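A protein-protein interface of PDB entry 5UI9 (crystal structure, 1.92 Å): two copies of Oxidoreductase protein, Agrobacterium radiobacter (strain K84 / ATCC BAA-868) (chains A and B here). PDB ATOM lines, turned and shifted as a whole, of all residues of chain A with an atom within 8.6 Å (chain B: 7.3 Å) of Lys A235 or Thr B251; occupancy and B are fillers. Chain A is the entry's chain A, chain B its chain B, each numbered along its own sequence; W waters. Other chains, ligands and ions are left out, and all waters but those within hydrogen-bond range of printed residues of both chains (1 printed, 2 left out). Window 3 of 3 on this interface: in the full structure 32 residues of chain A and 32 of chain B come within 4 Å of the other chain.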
ATOM      1  N   ARG A 156     -22.989  19.887 -14.417  1.00  0.00           N
ATOM      2  CA  ARG A 156     -23.628  19.494 -15.675  1.00  0.00           C
ATOM      3  C   ARG A 156     -22.537  19.418 -16.731  1.00  0.00           C
ATOM      4  O   ARG A 156     -21.860  20.408 -16.996  1.00  0.00           O
ATOM      5  CB  ARG A 156     -24.711  20.494 -16.089  1.00  0.00           C
ATOM      6  CG  ARG A 156     -25.712  20.826 -14.988  1.00  0.00           C
ATOM      7  CD  ARG A 156     -26.945  21.536 -15.545  1.00  0.00           C
ATOM      8  NE  ARG A 156     -27.847  20.579 -16.200  1.00  0.00           N
ATOM      9  CZ  ARG A 156     -28.657  19.728 -15.570  1.00  0.00           C
ATOM     10  NH1 ARG A 156     -28.710  19.676 -14.237  1.00  0.00           N
ATOM     11  NH2 ARG A 156     -29.417  18.897 -16.282  1.00  0.00           N
ATOM     12  N   SER A 157     -22.377  18.231 -17.306  1.00  0.00           N
ATOM     13  CA  SER A 157     -21.227  17.887 -18.133  1.00  0.00           C
ATOM     14  C   SER A 157     -21.638  16.974 -19.277  1.00  0.00           C
ATOM     15  O   SER A 157     -22.652  16.281 -19.190  1.00  0.00           O
ATOM     16  CB  SER A 157     -20.184  17.165 -17.277  1.00  0.00           C
ATOM     17  OG  SER A 157     -19.057  16.804 -18.047  1.00  0.00           O
ATOM     18  N   GLY A 158     -20.853  17.011 -20.349  1.00  0.00           N
ATOM     19  CA  GLY A 158     -20.929  16.035 -21.436  1.00  0.00           C
ATOM     20  C   GLY A 158     -19.622  15.272 -21.608  1.00  0.00           C
ATOM     21  O   GLY A 158     -19.376  14.711 -22.671  1.00  0.00           O
ATOM     22  N   PHE A 159     -18.803  15.228 -20.551  1.00  0.00           N
ATOM     23  CA  PHE A 159     -17.465  14.629 -20.605  1.00  0.00           C
ATOM     24  C   PHE A 159     -17.574  13.107 -20.660  1.00  0.00           C
ATOM     25  O   PHE A 159     -18.409  12.513 -19.973  1.00  0.00           O
ATOM     26  CB  PHE A 159     -16.650  15.051 -19.371  1.00  0.00           C
ATOM     27  CG  PHE A 159     -15.230  14.541 -19.361  1.00  0.00           C
ATOM     28  CD1 PHE A 159     -14.276  15.084 -20.216  1.00  0.00           C
ATOM     29  CD2 PHE A 159     -14.845  13.527 -18.484  1.00  0.00           C
ATOM     30  CE1 PHE A 159     -12.964  14.619 -20.205  1.00  0.00           C
ATOM     31  CE2 PHE A 159     -13.540  13.058 -18.469  1.00  0.00           C
ATOM     32  CZ  PHE A 159     -12.597  13.607 -19.327  1.00  0.00           C
ATOM     33  N   LYS A 202     -33.463  10.518 -14.474  1.00  0.00           N
ATOM     34  CA  LYS A 202     -33.755   9.911 -15.763  1.00  0.00           C
ATOM     35  C   LYS A 202     -32.481   9.479 -16.481  1.00  0.00           C
ATOM     36  O   LYS A 202     -31.370   9.863 -16.090  1.00  0.00           O
ATOM     37  CB  LYS A 202     -34.566  10.871 -16.644  1.00  0.00           C
ATOM     38  CG  LYS A 202     -33.883  12.185 -16.976  1.00  0.00           C
ATOM     39  CD  LYS A 202     -34.561  12.882 -18.149  1.00  0.00           C
ATOM     40  CE  LYS A 202     -35.971  13.353 -17.817  1.00  0.00           C
ATOM     41  NZ  LYS A 202     -36.012  14.334 -16.690  1.00  0.00           N
ATOM     42  N   ARG A 203     -32.662   8.676 -17.525  1.00  0.00           N
ATOM     43  CA  ARG A 203     -31.570   8.257 -18.401  1.00  0.00           C
ATOM     44  C   ARG A 203     -31.773   8.869 -19.774  1.00  0.00           C
ATOM     45  O   ARG A 203     -32.766   8.591 -20.421  1.00  0.00           O
ATOM     46  CB  ARG A 203     -31.506   6.736 -18.516  1.00  0.00           C
ATOM     47  CG  ARG A 203     -30.312   6.243 -19.320  1.00  0.00           C
ATOM     48  CD  ARG A 203     -30.133   4.744 -19.178  1.00  0.00           C
ATOM     49  NE  ARG A 203     -31.290   3.989 -19.655  1.00  0.00           N
ATOM     50  CZ  ARG A 203     -31.551   3.688 -20.927  1.00  0.00           C
ATOM     51  NH1 ARG A 203     -30.744   4.075 -21.919  1.00  0.00           N
ATOM     52  NH2 ARG A 203     -32.641   2.990 -21.212  1.00  0.00           N
ATOM     53  N   VAL A 204     -30.832   9.709 -20.199  1.00  0.00           N
ATOM     54  CA  VAL A 204     -30.828  10.292 -21.540  1.00  0.00           C
ATOM     55  C   VAL A 204     -29.942   9.482 -22.500  1.00  0.00           C
ATOM     56  O   VAL A 204     -30.367   9.144 -23.601  1.00  0.00           O
ATOM     57  CB  VAL A 204     -30.363  11.766 -21.499  1.00  0.00           C
ATOM     58  CG1 VAL A 204     -30.339  12.370 -22.907  1.00  0.00           C
ATOM     59  CG2 VAL A 204     -31.266  12.571 -20.572  1.00  0.00           C
ATOM     60  N   ASN A 205     -28.716   9.183 -22.074  1.00  0.00           N
ATOM     61  CA  ASN A 205     -27.729   8.482 -22.910  1.00  0.00           C
ATOM     62  C   ASN A 205     -28.209   7.053 -23.215  1.00  0.00           C
ATOM     63  O   ASN A 205     -28.397   6.255 -22.292  1.00  0.00           O
ATOM     64  CB  ASN A 205     -26.369   8.460 -22.190  1.00  0.00           C
ATOM     65  CG  ASN A 205     -25.216   7.980 -23.064  1.00  0.00           C
ATOM     66  OD1 ASN A 205     -25.398   7.281 -24.060  1.00  0.00           O
ATOM     67  ND2 ASN A 205     -24.006   8.355 -22.672  1.00  0.00           N
ATOM     68  N   PRO A 206     -28.405   6.725 -24.508  1.00  0.00           N
ATOM     69  CA  PRO A 206     -28.858   5.368 -24.854  1.00  0.00           C
ATOM     70  C   PRO A 206     -27.806   4.255 -24.678  1.00  0.00           C
ATOM     71  O   PRO A 206     -28.181   3.093 -24.644  1.00  0.00           O
ATOM     72  CB  PRO A 206     -29.278   5.500 -26.324  1.00  0.00           C
ATOM     73  CG  PRO A 206     -28.453   6.619 -26.855  1.00  0.00           C
ATOM     74  CD  PRO A 206     -28.205   7.562 -25.708  1.00  0.00           C
ATOM     75  N   SER A 231     -25.766  16.160 -14.109  1.00  0.00           N
ATOM     76  CA  SER A 231     -26.015  15.600 -15.428  1.00  0.00           C
ATOM     77  C   SER A 231     -24.703  15.238 -16.106  1.00  0.00           C
ATOM     78  O   SER A 231     -23.751  16.025 -16.055  1.00  0.00           O
ATOM     79  CB  SER A 231     -26.763  16.617 -16.301  1.00  0.00           C
ATOM     80  OG  SER A 231     -26.876  16.177 -17.653  1.00  0.00           O
ATOM     81  N   TYR A 232     -24.658  14.054 -16.716  1.00  0.00           N
ATOM     82  CA  TYR A 232     -23.596  13.674 -17.663  1.00  0.00           C
ATOM     83  C   TYR A 232     -24.108  13.619 -19.124  1.00  0.00           C
ATOM     84  O   TYR A 232     -23.455  13.029 -19.997  1.00  0.00           O
ATOM     85  CB  TYR A 232     -22.942  12.349 -17.248  1.00  0.00           C
ATOM     86  CG  TYR A 232     -21.703  12.513 -16.384  1.00  0.00           C
ATOM     87  CD1 TYR A 232     -20.602  13.254 -16.838  1.00  0.00           C
ATOM     88  CD2 TYR A 232     -21.615  11.922 -15.124  1.00  0.00           C
ATOM     89  CE1 TYR A 232     -19.460  13.395 -16.062  1.00  0.00           C
ATOM     90  CE2 TYR A 232     -20.477  12.068 -14.342  1.00  0.00           C
ATOM     91  CZ  TYR A 232     -19.407  12.802 -14.817  1.00  0.00           C
ATOM     92  OH  TYR A 232     -18.278  12.950 -14.053  1.00  0.00           O
ATOM     93  N   ALA A 233     -25.248  14.261 -19.391  1.00  0.00           N
ATOM     94  CA  ALA A 233     -25.813  14.350 -20.748  1.00  0.00           C
ATOM     95  C   ALA A 233     -26.021  15.807 -21.205  1.00  0.00           C
ATOM     96  O   ALA A 233     -26.872  16.083 -22.050  1.00  0.00           O
ATOM     97  CB  ALA A 233     -27.122  13.577 -20.810  1.00  0.00           C
ATOM     98  N   THR A 234     -25.222  16.724 -20.660  1.00  0.00           N
ATOM     99  CA  THR A 234     -25.342  18.147 -20.939  1.00  0.00           C
ATOM    100  C   THR A 234     -24.274  18.542 -21.967  1.00  0.00           C
ATOM    101  O   THR A 234     -23.082  18.357 -21.723  1.00  0.00           O
ATOM    102  CB  THR A 234     -25.208  18.955 -19.634  1.00  0.00           C
ATOM    103  OG1 THR A 234     -26.282  18.606 -18.749  1.00  0.00           O
ATOM    104  CG2 THR A 234     -25.257  20.459 -19.896  1.00  0.00           C
ATOM    105  N   LYS A 235     -24.704  19.086 -23.106  1.00  0.00           N
ATOM    106  CA  LYS A 235     -23.804  19.404 -24.229  1.00  0.00           C
ATOM    107  C   LYS A 235     -23.635  20.907 -24.363  1.00  0.00           C
ATOM    108  O   LYS A 235     -24.486  21.596 -24.951  1.00  0.00           O
ATOM    109  CB  LYS A 235     -24.345  18.804 -25.526  1.00  0.00           C
ATOM    110  CG  LYS A 235     -24.310  17.285 -25.509  1.00  0.00           C
ATOM    111  CD  LYS A 235     -25.219  16.657 -26.552  1.00  0.00           C
ATOM    112  CE  LYS A 235     -25.205  15.141 -26.406  1.00  0.00           C
ATOM    113  NZ  LYS A 235     -25.944  14.481 -27.508  1.00  0.00           N
ATOM    114  N   LEU A 236     -22.536  21.408 -23.808  1.00  0.00           N
ATOM    115  CA  LEU A 236     -22.245  22.841 -23.778  1.00  0.00           C
ATOM    116  C   LEU A 236     -21.112  23.172 -24.735  1.00  0.00           C
ATOM    117  O   LEU A 236     -20.280  22.321 -25.031  1.00  0.00           O
ATOM    118  CB  LEU A 236     -21.861  23.263 -22.361  1.00  0.00           C
ATOM    119  CG  LEU A 236     -22.990  23.219 -21.326  1.00  0.00           C
ATOM    120  CD1 LEU A 236     -22.422  23.086 -19.925  1.00  0.00           C
ATOM    121  CD2 LEU A 236     -23.872  24.451 -21.437  1.00  0.00           C
ATOM    122  N   GLY A 237     -21.074  24.418 -25.198  1.00  0.00           N
ATOM    123  CA  GLY A 237     -20.010  24.884 -26.104  1.00  0.00           C
ATOM    124  C   GLY A 237     -18.618  24.720 -25.498  1.00  0.00           C
ATOM    125  O   GLY A 237     -17.679  24.309 -26.178  1.00  0.00           O
ATOM    126  N   THR A 238     -18.494  25.041 -24.214  1.00  0.00           N
ATOM    127  CA  THR A 238     -17.273  24.781 -23.460  1.00  0.00           C
ATOM    128  C   THR A 238     -17.581  23.719 -22.429  1.00  0.00           C
ATOM    129  O   THR A 238     -18.458  23.921 -21.588  1.00  0.00           O
ATOM    130  CB  THR A 238     -16.774  26.045 -22.746  1.00  0.00           C
ATOM    131  OG1 THR A 238     -16.551  27.070 -23.713  1.00  0.00           O
ATOM    132  CG2 THR A 238     -15.464  25.768 -21.967  1.00  0.00           C
ATOM    133  N   GLU A 239     -16.858  22.601 -22.493  1.00  0.00           N
ATOM    134  CA  GLU A 239     -17.027  21.499 -21.541  1.00  0.00           C
ATOM    135  C   GLU A 239     -16.540  21.926 -20.149  1.00  0.00           C
ATOM    136  O   GLU A 239     -15.347  22.158 -19.967  1.00  0.00           O
ATOM    137  CB  GLU A 239     -16.257  20.254 -22.024  1.00  0.00           C
ATOM    138  CG  GLU A 239     -16.268  19.051 -21.078  1.00  0.00           C
ATOM    139  CD  GLU A 239     -17.652  18.723 -20.545  1.00  0.00           C
ATOM    140  OE1 GLU A 239     -18.569  18.480 -21.358  1.00  0.00           O
ATOM    141  OE2 GLU A 239     -17.826  18.718 -19.305  1.00  0.00           O
ATOM    142  N   PRO A 240     -17.456  22.024 -19.161  1.00  0.00           N
ATOM    143  CA  PRO A 240     -17.019  22.487 -17.838  1.00  0.00           C
ATOM    144  C   PRO A 240     -16.347  21.454 -16.911  1.00  0.00           C
ATOM    145  O   PRO A 240     -15.916  21.846 -15.828  1.00  0.00           O
ATOM    146  CB  PRO A 240     -18.329  22.958 -17.203  1.00  0.00           C
ATOM    147  CG  PRO A 240     -19.333  22.048 -17.776  1.00  0.00           C
ATOM    148  CD  PRO A 240     -18.919  21.851 -19.203  1.00  0.00           C
ATOM    149  N   GLY B 143     -35.827  22.565 -33.102  1.00  0.00           N
ATOM    150  CA  GLY B 143     -35.195  21.251 -32.980  1.00  0.00           C
ATOM    151  C   GLY B 143     -33.687  21.334 -32.853  1.00  0.00           C
ATOM    152  O   GLY B 143     -33.006  20.317 -32.945  1.00  0.00           O
ATOM    153  N   ILE B 145     -31.674  21.838 -30.352  1.00  0.00           N
ATOM    154  CA  ILE B 145     -31.057  21.111 -29.230  1.00  0.00           C
ATOM    155  C   ILE B 145     -31.699  19.739 -28.971  1.00  0.00           C
ATOM    156  O   ILE B 145     -31.455  19.117 -27.926  1.00  0.00           O
ATOM    157  CB  ILE B 145     -31.033  21.965 -27.948  1.00  0.00           C
ATOM    158  CG1 ILE B 145     -32.435  22.237 -27.401  1.00  0.00           C
ATOM    159  CG2 ILE B 145     -30.302  23.277 -28.203  1.00  0.00           C
ATOM    160  CD1 ILE B 145     -32.415  22.637 -25.939  1.00  0.00           C
ATOM    161  N   GLY B 146     -32.469  19.249 -29.940  1.00  0.00           N
ATOM    162  CA  GLY B 146     -33.212  18.001 -29.792  1.00  0.00           C
ATOM    163  C   GLY B 146     -34.369  18.127 -28.816  1.00  0.00           C
ATOM    164  O   GLY B 146     -34.943  19.210 -28.660  1.00  0.00           O
ATOM    165  N   GLU B 147     -34.705  17.018 -28.160  1.00  0.00           N
ATOM    166  CA  GLU B 147     -35.832  16.973 -27.224  1.00  0.00           C
ATOM    167  C   GLU B 147     -35.367  17.477 -25.853  1.00  0.00           C
ATOM    168  O   GLU B 147     -34.366  16.997 -25.342  1.00  0.00           O
ATOM    169  CB  GLU B 147     -36.359  15.541 -27.085  1.00  0.00           C
ATOM    170  CG  GLU B 147     -36.816  14.890 -28.393  1.00  0.00           C
ATOM    171  CD  GLU B 147     -38.272  15.176 -28.743  1.00  0.00           C
ATOM    172  OE1 GLU B 147     -38.783  16.286 -28.447  1.00  0.00           O
ATOM    173  OE2 GLU B 147     -38.914  14.277 -29.332  1.00  0.00           O
ATOM    174  N   PRO B 148     -36.091  18.436 -25.254  1.00  0.00           N
ATOM    175  CA  PRO B 148     -35.671  18.946 -23.951  1.00  0.00           C
ATOM    176  C   PRO B 148     -35.932  17.938 -22.831  1.00  0.00           C
ATOM    177  O   PRO B 148     -36.969  17.275 -22.841  1.00  0.00           O
ATOM    178  CB  PRO B 148     -36.551  20.184 -23.764  1.00  0.00           C
ATOM    179  CG  PRO B 148     -37.794  19.876 -24.542  1.00  0.00           C
ATOM    180  CD  PRO B 148     -37.375  19.018 -25.689  1.00  0.00           C
ATOM    181  N   PHE B 149     -34.996  17.812 -21.891  1.00  0.00           N
ATOM    182  CA  PHE B 149     -35.188  16.945 -20.710  1.00  0.00           C
ATOM    183  C   PHE B 149     -35.038  17.632 -19.346  1.00  0.00           C
ATOM    184  O   PHE B 149     -35.443  17.067 -18.321  1.00  0.00           O
ATOM    185  CB  PHE B 149     -34.301  15.687 -20.802  1.00  0.00           C
ATOM    186  CG  PHE B 149     -32.816  15.953 -20.751  1.00  0.00           C
ATOM    187  CD1 PHE B 149     -32.158  16.124 -19.528  1.00  0.00           C
ATOM    188  CD2 PHE B 149     -32.064  15.984 -21.918  1.00  0.00           C
ATOM    189  CE1 PHE B 149     -30.793  16.352 -19.479  1.00  0.00           C
ATOM    190  CE2 PHE B 149     -30.700  16.215 -21.875  1.00  0.00           C
ATOM    191  CZ  PHE B 149     -30.060  16.392 -20.654  1.00  0.00           C
ATOM    192  N   ILE B 248     -31.847  25.355 -20.553  1.00  0.00           N
ATOM    193  CA  ILE B 248     -32.527  24.158 -21.042  1.00  0.00           C
ATOM    194  C   ILE B 248     -31.458  23.185 -21.506  1.00  0.00           C
ATOM    195  O   ILE B 248     -30.513  23.591 -22.187  1.00  0.00           O
ATOM    196  CB  ILE B 248     -33.476  24.437 -22.241  1.00  0.00           C
ATOM    197  CG1 ILE B 248     -34.438  25.601 -21.971  1.00  0.00           C
ATOM    198  CG2 ILE B 248     -34.270  23.185 -22.606  1.00  0.00           C
ATOM    199  CD1 ILE B 248     -35.504  25.327 -20.934  1.00  0.00           C
ATOM    200  N   ASP B 249     -31.609  21.911 -21.141  1.00  0.00           N
ATOM    201  CA  ASP B 249     -30.771  20.833 -21.684  1.00  0.00           C
ATOM    202  C   ASP B 249     -31.647  19.919 -22.534  1.00  0.00           C
ATOM    203  O   ASP B 249     -32.758  19.540 -22.122  1.00  0.00           O
ATOM    204  CB  ASP B 249     -30.108  20.014 -20.574  1.00  0.00           C
ATOM    205  CG  ASP B 249     -29.065  20.799 -19.784  1.00  0.00           C
ATOM    206  OD1 ASP B 249     -28.856  22.014 -20.033  1.00  0.00           O
ATOM    207  OD2 ASP B 249     -28.463  20.181 -18.880  1.00  0.00           O
ATOM    208  N   GLY B 250     -31.143  19.575 -23.716  1.00  0.00           N
ATOM    209  CA  GLY B 250     -31.829  18.682 -24.631  1.00  0.00           C
ATOM    210  C   GLY B 250     -30.909  17.583 -25.090  1.00  0.00           C
ATOM    211  O   GLY B 250     -29.703  17.640 -24.855  1.00  0.00           O
ATOM    212  N   THR B 251     -31.476  16.594 -25.772  1.00  0.00           N
ATOM    213  CA  THR B 251     -30.722  15.430 -26.246  1.00  0.00           C
ATOM    214  C   THR B 251     -29.561  15.759 -27.187  1.00  0.00           C
ATOM    215  O   THR B 251     -28.598  15.003 -27.243  1.00  0.00           O
ATOM    216  CB  THR B 251     -31.637  14.410 -26.959  1.00  0.00           C
ATOM    217  OG1 THR B 251     -32.388  15.074 -27.983  1.00  0.00           O
ATOM    218  CG2 THR B 251     -32.601  13.762 -25.968  1.00  0.00           C
ATOM    219  N   GLN B 252     -29.648  16.872 -27.918  1.00  0.00           N
ATOM    220  CA  GLN B 252     -28.605  17.266 -28.885  1.00  0.00           C
ATOM    221  C   GLN B 252     -27.939  18.618 -28.565  1.00  0.00           C
ATOM    222  O   GLN B 252     -27.132  19.107 -29.356  1.00  0.00           O
ATOM    223  CB  GLN B 252     -29.198  17.313 -30.299  1.00  0.00           C
ATOM    224  CG  GLN B 252     -29.706  15.977 -30.817  1.00  0.00           C
ATOM    225  CD  GLN B 252     -30.338  16.076 -32.205  1.00  0.00           C
ATOM    226  OE1 GLN B 252     -30.545  17.167 -32.743  1.00  0.00           O
ATOM    227  NE2 GLN B 252     -30.642  14.925 -32.793  1.00  0.00           N
ATOM    228  N   GLY B 253     -28.257  19.225 -27.422  1.00  0.00           N
ATOM    229  CA  GLY B 253     -27.714  20.542 -27.125  1.00  0.00           C
ATOM    230  C   GLY B 253     -28.231  21.236 -25.884  1.00  0.00           C
ATOM    231  O   GLY B 253     -28.894  20.624 -25.035  1.00  0.00           O
ATOM    232  N   THR B 254     -27.915  22.528 -25.795  1.00  0.00           N
ATOM    233  CA  THR B 254     -28.293  23.359 -24.664  1.00  0.00           C
ATOM    234  C   THR B 254     -28.656  24.769 -25.087  1.00  0.00           C
ATOM    235  O   THR B 254     -28.120  25.288 -26.066  1.00  0.00           O
ATOM    236  CB  THR B 254     -27.146  23.478 -23.632  1.00  0.00           C
ATOM    237  OG1 THR B 254     -25.946  23.903 -24.284  1.00  0.00           O
ATOM    238  CG2 THR B 254     -26.904  22.154 -22.931  1.00  0.00           C
ATOM    239  N   ILE B 255     -29.562  25.369 -24.321  1.00  0.00           N
ATOM    240  CA  ILE B 255     -29.858  26.787 -24.363  1.00  0.00           C
ATOM    241  C   ILE B 255     -29.454  27.385 -23.007  1.00  0.00           C
ATOM    242  O   ILE B 255     -29.760  26.813 -21.955  1.00  0.00           O
ATOM    243  CB  ILE B 255     -31.363  27.031 -24.619  1.00  0.00           C
ATOM    244  CG1 ILE B 255     -31.746  26.569 -26.032  1.00  0.00           C
ATOM    245  CG2 ILE B 255     -31.729  28.498 -24.418  1.00  0.00           C
ATOM    246  CD1 ILE B 255     -33.229  26.349 -26.228  1.00  0.00           C
ATOM    247  N   ARG B 256     -28.749  28.519 -23.052  1.00  0.00           N
ATOM    248  CA  ARG B 256     -28.366  29.288 -21.866  1.00  0.00           C
ATOM    249  C   ARG B 256     -28.646  30.772 -22.139  1.00  0.00           C
ATOM    250  O   ARG B 256     -27.902  31.441 -22.881  1.00  0.00           O
ATOM    251  CB  ARG B 256     -26.889  29.075 -21.512  1.00  0.00           C
ATOM    252  CG  ARG B 256     -26.508  27.658 -21.080  1.00  0.00           C
ATOM    253  CD  ARG B 256     -27.011  27.340 -19.682  1.00  0.00           C
ATOM    254  NE  ARG B 256     -26.603  26.015 -19.201  1.00  0.00           N
ATOM    255  CZ  ARG B 256     -27.173  24.847 -19.532  1.00  0.00           C
ATOM    256  NH1 ARG B 256     -28.199  24.785 -20.386  1.00  0.00           N
ATOM    257  NH2 ARG B 256     -26.709  23.715 -18.997  1.00  0.00           N
ATOM    258  N   GLU B 264     -27.135  31.844 -25.566  1.00  0.00           N
ATOM    259  CA  GLU B 264     -26.117  30.920 -26.053  1.00  0.00           C
ATOM    260  C   GLU B 264     -26.786  29.593 -26.399  1.00  0.00           C
ATOM    261  O   GLU B 264     -27.521  29.046 -25.585  1.00  0.00           O
ATOM    262  CB  GLU B 264     -25.051  30.720 -24.973  1.00  0.00           C
ATOM    263  CG  GLU B 264     -23.896  29.818 -25.367  1.00  0.00           C
ATOM    264  CD  GLU B 264     -22.957  29.551 -24.199  1.00  0.00           C
ATOM    265  OE1 GLU B 264     -22.982  28.399 -23.658  1.00  0.00           O
ATOM    266  OE2 GLU B 264     -22.235  30.506 -23.815  1.00  0.00           O
ATOM    267  N   VAL B 265     -26.533  29.079 -27.598  1.00  0.00           N
ATOM    268  CA  VAL B 265     -27.145  27.835 -28.051  1.00  0.00           C
ATOM    269  C   VAL B 265     -26.051  26.933 -28.576  1.00  0.00           C
ATOM    270  O   VAL B 265     -25.336  27.316 -29.498  1.00  0.00           O
ATOM    271  CB  VAL B 265     -28.202  28.076 -29.161  1.00  0.00           C
ATOM    272  CG1 VAL B 265     -28.813  26.757 -29.642  1.00  0.00           C
ATOM    273  CG2 VAL B 265     -29.287  29.029 -28.662  1.00  0.00           C
ATOM    274  N   THR B 266     -25.903  25.755 -27.971  1.00  0.00           N
ATOM    275  CA  THR B 266     -24.962  24.736 -28.456  1.00  0.00           C
ATOM    276  C   THR B 266     -25.796  23.612 -29.031  1.00  0.00           C
ATOM    277  O   THR B 266     -26.752  23.158 -28.403  1.00  0.00           O
ATOM    278  CB  THR B 266     -24.071  24.171 -27.328  1.00  0.00           C
ATOM    279  OG1 THR B 266     -23.418  25.244 -26.640  1.00  0.00           O
ATOM    280  CG2 THR B 266     -23.015  23.205 -27.879  1.00  0.00           C
ATOM    281  N   GLY B 267     -25.455  23.198 -30.243  1.00  0.00           N
ATOM    282  CA  GLY B 267     -26.130  22.105 -30.933  1.00  0.00           C
ATOM    283  C   GLY B 267     -25.092  21.219 -31.592  1.00  0.00           C
ATOM    284  O   GLY B 267     -23.898  21.364 -31.321  1.00  0.00           O
ATOM    285  N   PRO B 268     -25.536  20.293 -32.460  1.00  0.00           N
ATOM    286  CA  PRO B 268     -24.581  19.427 -33.165  1.00  0.00           C
ATOM    287  C   PRO B 268     -23.602  20.208 -34.064  1.00  0.00           C
ATOM    288  O   PRO B 268     -22.427  19.832 -34.153  1.00  0.00           O
ATOM    289  CB  PRO B 268     -25.486  18.502 -34.001  1.00  0.00           C
ATOM    290  CG  PRO B 268     -26.836  18.593 -33.368  1.00  0.00           C
ATOM    291  CD  PRO B 268     -26.933  19.979 -32.812  1.00  0.00           C
ATOM    292  N   GLY B 270     -22.092  23.156 -33.690  1.00  0.00           N
ATOM    293  CA  GLY B 270     -21.357  24.195 -32.978  1.00  0.00           C
ATOM    294  C   GLY B 270     -22.181  24.995 -31.993  1.00  0.00           C
ATOM    295  O   GLY B 270     -23.152  24.494 -31.412  1.00  0.00           O
HETATM  296  O   HOH W   1     -20.645  26.755 -23.012  1.00  0.00           O
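N of Gly A158 sits at hydrogen-bond distance from O of Thr A234, 2.9 Å away.
The side-chain hydroxyl of Ser A231 lies within hydrogen-bond range of the side-chain hydroxyl of Thr A234 (2.7 Å).
The backbone carbonyl oxygen (O) of Ile B145 is in hydrogen-bond range of the backbone NH (N) of Gly B253 (3.2 Å).
N of Phe B149 sits at hydrogen-bond distance from O of Asp B249, at 2.8 Å.
The guanidinium group of Arg B256 lies within salt-bridge range of the side-chain carboxylate of Asp B249, 2.9 Å away.
O of Arg B256 sits at hydrogen-bond distance from N of Glu B264 (2.8 Å).
Water W1 lies within hydrogen-bond range of OE1 of Glu B264 (2.9 Å), N of Thr A238 (3.0 Å) and N of Gly A237 (3.2 Å).
Lys A235 touches just these residues of chain B: Thr B251 (2.7 Å), Gln B252 (3.9 Å), Gly B253 (3.9 Å), Thr B254 (2.8 Å) and Thr B266 (3.5 Å).
Of chain A, only Lys A235 comes within 4 Å of Thr B251.
Of the printed residues of chain B, Val A204 touches Phe B149.
Printed residues of chain A within 4 Å of Gln B252: Lys A235.
The nearest printed residue of chain A that does not touch Thr B254 is Gly A237 (5.0 Å).
Hydrophobic or aromatic side chains of chain A within 4 Å of the printed part of chain B: Val A204 and Leu A236.
Of the 21 printed residues of chain B, 8 touch a printed residue of chain A.
Val A204 touches Phe B149 (CG2 to CG, 3.7 Å).
Ala A233 touches Phe B149 (O to CZ, 3.5 Å).
Thr A234 touches Thr B254.
Thr A234 touches Arg B256 (CG2 to NH2, 3.7 Å).
CD of Lys A235 touches C of Gln B252 (3.9 Å).
C of Gly B253 touches O of Lys A235, 3.9 Å away.
Lys A235 touches Thr B266 (O to CB, 3.5 Å).
Thr B254 touches Leu A236.
Arg B256 touches Leu A236.
Leu A236 touches Thr B266 (C to OG1, 3.6 Å).
No position is printed for both chains.
Of the 16 pairs that touch across the chains among the printed residues, none has its exchanged pair printed and touching as well.
The guanidinium group (NE) of Arg A156 lies within salt-bridge range of the side-chain carboxylate (OD2) of Asp B249, 2.8 Å away.
The side-chain amino group of Lys A202 sits at hydrogen-bond distance from the backbone carbonyl oxygen of Phe B149 (3.2 Å).
OD2 of Asp B249 lies within hydrogen-bond range of OG1 of Thr A234 (2.7 Å).
The side-chain amino group of Lys A235 lies within hydrogen-bond range of the backbone carbonyl oxygen of Thr B251, 2.7 Å away.
O of Lys A235 is in hydrogen-bond range of OG1 of Thr B254.
The side-chain hydroxyl (OG1) of Thr B266 is in hydrogen-bond range of the backbone NH (N) of Gly A237 (2.9 Å).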
